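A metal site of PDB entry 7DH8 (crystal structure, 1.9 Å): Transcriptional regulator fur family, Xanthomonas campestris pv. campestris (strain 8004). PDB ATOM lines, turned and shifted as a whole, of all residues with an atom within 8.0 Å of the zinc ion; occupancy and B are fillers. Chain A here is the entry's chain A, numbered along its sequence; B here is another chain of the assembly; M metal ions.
The side-chain sulfur (SG) of Cys 126 binds the zinc ion, 2.2 Å away.
SG of Cys 123 is bound to the zinc ion (2.3 Å).
The side-chain sulfur (SG) of Cys 163 binds the zinc ion, at 2.4 Å.
The zinc ion is bound by SG of Cys 166, at 2.4 Å.
The zinc ion has four donor atoms within binding distance.
The backbone NH of Arg 125 lies close to the side-chain sulfur of Cys 123 (3.4 Å).
The side-chain hydroxyl (OG) of Ser 128 lies close to the side-chain sulfur (SG) of Cys 126 (3.5 Å).
The backbone carbonyl oxygen (O) of Cys 166 sits at hydrogen-bond distance from the guanidinium group (NH1) of Arg 125 (3.4 Å).
The backbone NH (N) of Cys 123 sits at hydrogen-bond distance from the backbone carbonyl oxygen (O) of Ser 128.
SG of Cys 163 lies close to N of Lys 165, 3.6 Å away.
The side-chain amino group (NZ) of Lys 58 sits at hydrogen-bond distance from the backbone carbonyl oxygen (O) of Cys 126.
Of the 17 residues printed, 4 come within 4 Å of the zinc ion.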
ATOM      1  N   LYS A  58      10.389  -7.105  21.491  1.00  0.00           N
ATOM      2  CA  LYS A  58       9.878  -7.960  20.449  1.00  0.00           C
ATOM      3  C   LYS A  58      10.655  -7.567  19.203  1.00  0.00           C
ATOM      4  O   LYS A  58      11.238  -6.463  19.177  1.00  0.00           O
ATOM      5  CB  LYS A  58       8.364  -7.761  20.216  1.00  0.00           C
ATOM      6  CG  LYS A  58       7.454  -8.196  21.349  1.00  0.00           C
ATOM      7  CD  LYS A  58       6.986  -9.662  21.243  1.00  0.00           C
ATOM      8  CE  LYS A  58       6.082 -10.051  22.448  1.00  0.00           C
ATOM      9  NZ  LYS A  58       4.623  -9.927  22.055  1.00  0.00           N
ATOM     10  N   ILE A 122      10.996 -18.618  17.660  1.00  0.00           N
ATOM     11  CA  ILE A 122      10.138 -17.488  17.345  1.00  0.00           C
ATOM     12  C   ILE A 122       8.702 -17.940  17.523  1.00  0.00           C
ATOM     13  O   ILE A 122       8.268 -18.866  16.858  1.00  0.00           O
ATOM     14  CB  ILE A 122      10.404 -16.937  15.932  1.00  0.00           C
ATOM     15  CG1 ILE A 122      11.851 -16.520  15.793  1.00  0.00           C
ATOM     16  CG2 ILE A 122       9.511 -15.656  15.642  1.00  0.00           C
ATOM     17  CD1 ILE A 122      12.211 -16.199  14.249  1.00  0.00           C
ATOM     18  N   CYS A 123       7.984 -17.325  18.471  1.00  0.00           N
ATOM     19  CA  CYS A 123       6.643 -17.794  18.745  1.00  0.00           C
ATOM     20  C   CYS A 123       5.758 -17.327  17.602  1.00  0.00           C
ATOM     21  O   CYS A 123       5.780 -16.143  17.261  1.00  0.00           O
ATOM     22  CB  CYS A 123       6.127 -17.270  20.087  1.00  0.00           C
ATOM     23  SG  CYS A 123       4.450 -17.754  20.432  1.00  0.00           S
ATOM     24  N   ASP A 124       4.939 -18.235  17.068  1.00  0.00           N
ATOM     25  CA  ASP A 124       4.013 -17.871  16.012  1.00  0.00           C
ATOM     26  C   ASP A 124       2.939 -16.888  16.484  1.00  0.00           C
ATOM     27  O   ASP A 124       2.421 -16.131  15.680  1.00  0.00           O
ATOM     28  CB  ASP A 124       3.310 -19.122  15.469  1.00  0.00           C
ATOM     29  CG  ASP A 124       4.258 -20.076  14.753  1.00  0.00           C
ATOM     30  OD1 ASP A 124       5.380 -19.672  14.346  1.00  0.00           O
ATOM     31  OD2 ASP A 124       3.854 -21.247  14.571  1.00  0.00           O
ATOM     32  N   ARG A 125       2.565 -16.913  17.771  1.00  0.00           N
ATOM     33  CA  ARG A 125       1.386 -16.153  18.193  1.00  0.00           C
ATOM     34  C   ARG A 125       1.751 -14.783  18.773  1.00  0.00           C
ATOM     35  O   ARG A 125       1.193 -13.762  18.368  1.00  0.00           O
ATOM     36  CB  ARG A 125       0.588 -17.007  19.190  1.00  0.00           C
ATOM     37  CG  ARG A 125      -0.679 -16.274  19.788  1.00  0.00           C
ATOM     38  CD  ARG A 125      -1.626 -17.250  20.463  1.00  0.00           C
ATOM     39  NE  ARG A 125      -1.833 -18.421  19.641  1.00  0.00           N
ATOM     40  CZ  ARG A 125      -2.014 -19.635  20.157  1.00  0.00           C
ATOM     41  NH1 ARG A 125      -2.036 -19.756  21.476  1.00  0.00           N
ATOM     42  NH2 ARG A 125      -2.176 -20.697  19.362  1.00  0.00           N
ATOM     43  N   CYS A 126       2.713 -14.715  19.683  1.00  0.00           N
ATOM     44  CA  CYS A 126       3.063 -13.467  20.360  1.00  0.00           C
ATOM     45  C   CYS A 126       4.300 -12.826  19.774  1.00  0.00           C
ATOM     46  O   CYS A 126       4.653 -11.699  20.175  1.00  0.00           O
ATOM     47  CB  CYS A 126       3.269 -13.722  21.863  1.00  0.00           C
ATOM     48  SG  CYS A 126       4.828 -14.575  22.335  1.00  0.00           S
ATOM     49  N   HIS A 127       4.986 -13.534  18.855  1.00  0.00           N
ATOM     50  CA  HIS A 127       6.128 -13.075  18.058  1.00  0.00           C
ATOM     51  C   HIS A 127       7.388 -12.866  18.885  1.00  0.00           C
ATOM     52  O   HIS A 127       8.334 -12.253  18.368  1.00  0.00           O
ATOM     53  CB  HIS A 127       5.801 -11.773  17.275  1.00  0.00           C
ATOM     54  CG  HIS A 127       4.460 -11.819  16.586  1.00  0.00           C
ATOM     55  ND1 HIS A 127       3.415 -10.964  16.902  1.00  0.00           N
ATOM     56  CD2 HIS A 127       3.964 -12.684  15.668  1.00  0.00           C
ATOM     57  CE1 HIS A 127       2.354 -11.277  16.183  1.00  0.00           C
ATOM     58  NE2 HIS A 127       2.665 -12.306  15.410  1.00  0.00           N
ATOM     59  N   SER A 128       7.439 -13.311  20.136  1.00  0.00           N
ATOM     60  CA  SER A 128       8.706 -13.251  20.856  1.00  0.00           C
ATOM     61  C   SER A 128       9.756 -14.079  20.118  1.00  0.00           C
ATOM     62  O   SER A 128       9.434 -15.074  19.445  1.00  0.00           O
ATOM     63  CB  SER A 128       8.602 -13.813  22.288  1.00  0.00           C
ATOM     64  OG  SER A 128       8.245 -15.202  22.199  1.00  0.00           O
ATOM     65  N   ALA A 129      11.040 -13.698  20.327  1.00  0.00           N
ATOM     66  CA  ALA A 129      12.149 -14.401  19.698  1.00  0.00           C
ATOM     67  C   ALA A 129      13.231 -14.633  20.731  1.00  0.00           C
ATOM     68  O   ALA A 129      13.677 -13.700  21.416  1.00  0.00           O
ATOM     69  CB  ALA A 129      12.720 -13.635  18.516  1.00  0.00           C
ATOM     70  N   GLY A 161       6.682 -22.212  16.203  1.00  0.00           N
ATOM     71  CA  GLY A 161       5.799 -22.905  17.137  1.00  0.00           C
ATOM     72  C   GLY A 161       5.289 -21.890  18.155  1.00  0.00           C
ATOM     73  O   GLY A 161       5.169 -20.675  17.857  1.00  0.00           O
ATOM     74  N   LEU A 162       5.066 -22.372  19.377  1.00  0.00           N
ATOM     75  CA  LEU A 162       4.478 -21.551  20.433  1.00  0.00           C
ATOM     76  C   LEU A 162       5.393 -21.489  21.646  1.00  0.00           C
ATOM     77  O   LEU A 162       5.881 -22.538  22.118  1.00  0.00           O
ATOM     78  CB  LEU A 162       3.128 -22.103  20.862  1.00  0.00           C
ATOM     79  CG  LEU A 162       2.036 -22.088  19.759  1.00  0.00           C
ATOM     80  CD1 LEU A 162       0.748 -22.799  20.233  1.00  0.00           C
ATOM     81  CD2 LEU A 162       1.765 -20.668  19.232  1.00  0.00           C
ATOM     82  N   CYS A 163       5.586 -20.287  22.181  1.00  0.00           N
ATOM     83  CA  CYS A 163       6.341 -20.199  23.424  1.00  0.00           C
ATOM     84  C   CYS A 163       5.517 -20.790  24.582  1.00  0.00           C
ATOM     85  O   CYS A 163       4.343 -21.135  24.433  1.00  0.00           O
ATOM     86  CB  CYS A 163       6.743 -18.765  23.698  1.00  0.00           C
ATOM     87  SG  CYS A 163       5.232 -17.762  24.314  1.00  0.00           S
ATOM     88  N   ALA A 164       6.179 -21.007  25.735  1.00  0.00           N
ATOM     89  CA  ALA A 164       5.507 -21.637  26.872  1.00  0.00           C
ATOM     90  C   ALA A 164       4.245 -20.894  27.261  1.00  0.00           C
ATOM     91  O   ALA A 164       3.224 -21.520  27.566  1.00  0.00           O
ATOM     92  CB  ALA A 164       6.402 -21.701  28.091  1.00  0.00           C
ATOM     93  N   LYS A 165       4.306 -19.569  27.298  1.00  0.00           N
ATOM     94  CA  LYS A 165       3.106 -18.798  27.715  1.00  0.00           C
ATOM     95  C   LYS A 165       1.933 -19.063  26.773  1.00  0.00           C
ATOM     96  O   LYS A 165       0.809 -19.328  27.217  1.00  0.00           O
ATOM     97  CB  LYS A 165       3.415 -17.286  27.686  1.00  0.00           C
ATOM     98  CG  LYS A 165       4.056 -16.737  28.896  1.00  0.00           C
ATOM     99  CD  LYS A 165       5.511 -17.128  29.106  1.00  0.00           C
ATOM    100  CE  LYS A 165       6.098 -16.191  30.165  1.00  0.00           C
ATOM    101  NZ  LYS A 165       5.996 -14.776  29.635  1.00  0.00           N
ATOM    102  N   CYS A 166       2.182 -18.984  25.462  1.00  0.00           N
ATOM    103  CA  CYS A 166       1.090 -19.176  24.516  1.00  0.00           C
ATOM    104  C   CYS A 166       0.607 -20.614  24.471  1.00  0.00           C
ATOM    105  O   CYS A 166      -0.596 -20.847  24.319  1.00  0.00           O
ATOM    106  CB  CYS A 166       1.513 -18.706  23.116  1.00  0.00           C
ATOM    107  SG  CYS A 166       1.802 -16.882  22.948  1.00  0.00           S
ATOM    108  N   ALA A 167       1.521 -21.591  24.590  1.00  0.00           N
ATOM    109  CA  ALA A 167       1.080 -22.982  24.628  1.00  0.00           C
ATOM    110  C   ALA A 167       0.198 -23.267  25.831  1.00  0.00           C
ATOM    111  O   ALA A 167      -0.674 -24.136  25.773  1.00  0.00           O
ATOM    112  CB  ALA A 167       2.291 -23.905  24.627  1.00  0.00           C
ATOM    113  N   PHE B 150       9.322 -24.210  24.985  1.00  0.00           N
ATOM    114  CA  PHE B 150       8.782 -23.826  23.682  1.00  0.00           C
ATOM    115  C   PHE B 150       8.265 -25.066  22.947  1.00  0.00           C
ATOM    116  O   PHE B 150       8.940 -26.092  22.916  1.00  0.00           O
ATOM    117  CB  PHE B 150       9.899 -23.118  22.912  1.00  0.00           C
ATOM    118  CG  PHE B 150       9.476 -22.474  21.599  1.00  0.00           C
ATOM    119  CD1 PHE B 150       9.486 -23.197  20.411  1.00  0.00           C
ATOM    120  CD2 PHE B 150       9.160 -21.143  21.563  1.00  0.00           C
ATOM    121  CE1 PHE B 150       9.141 -22.568  19.194  1.00  0.00           C
ATOM    122  CE2 PHE B 150       8.802 -20.525  20.363  1.00  0.00           C
ATOM    123  CZ  PHE B 150       8.824 -21.241  19.195  1.00  0.00           C
HETATM  124 ZN    ZN M   1       4.153 -16.697  22.500  1.00  0.00          ZN
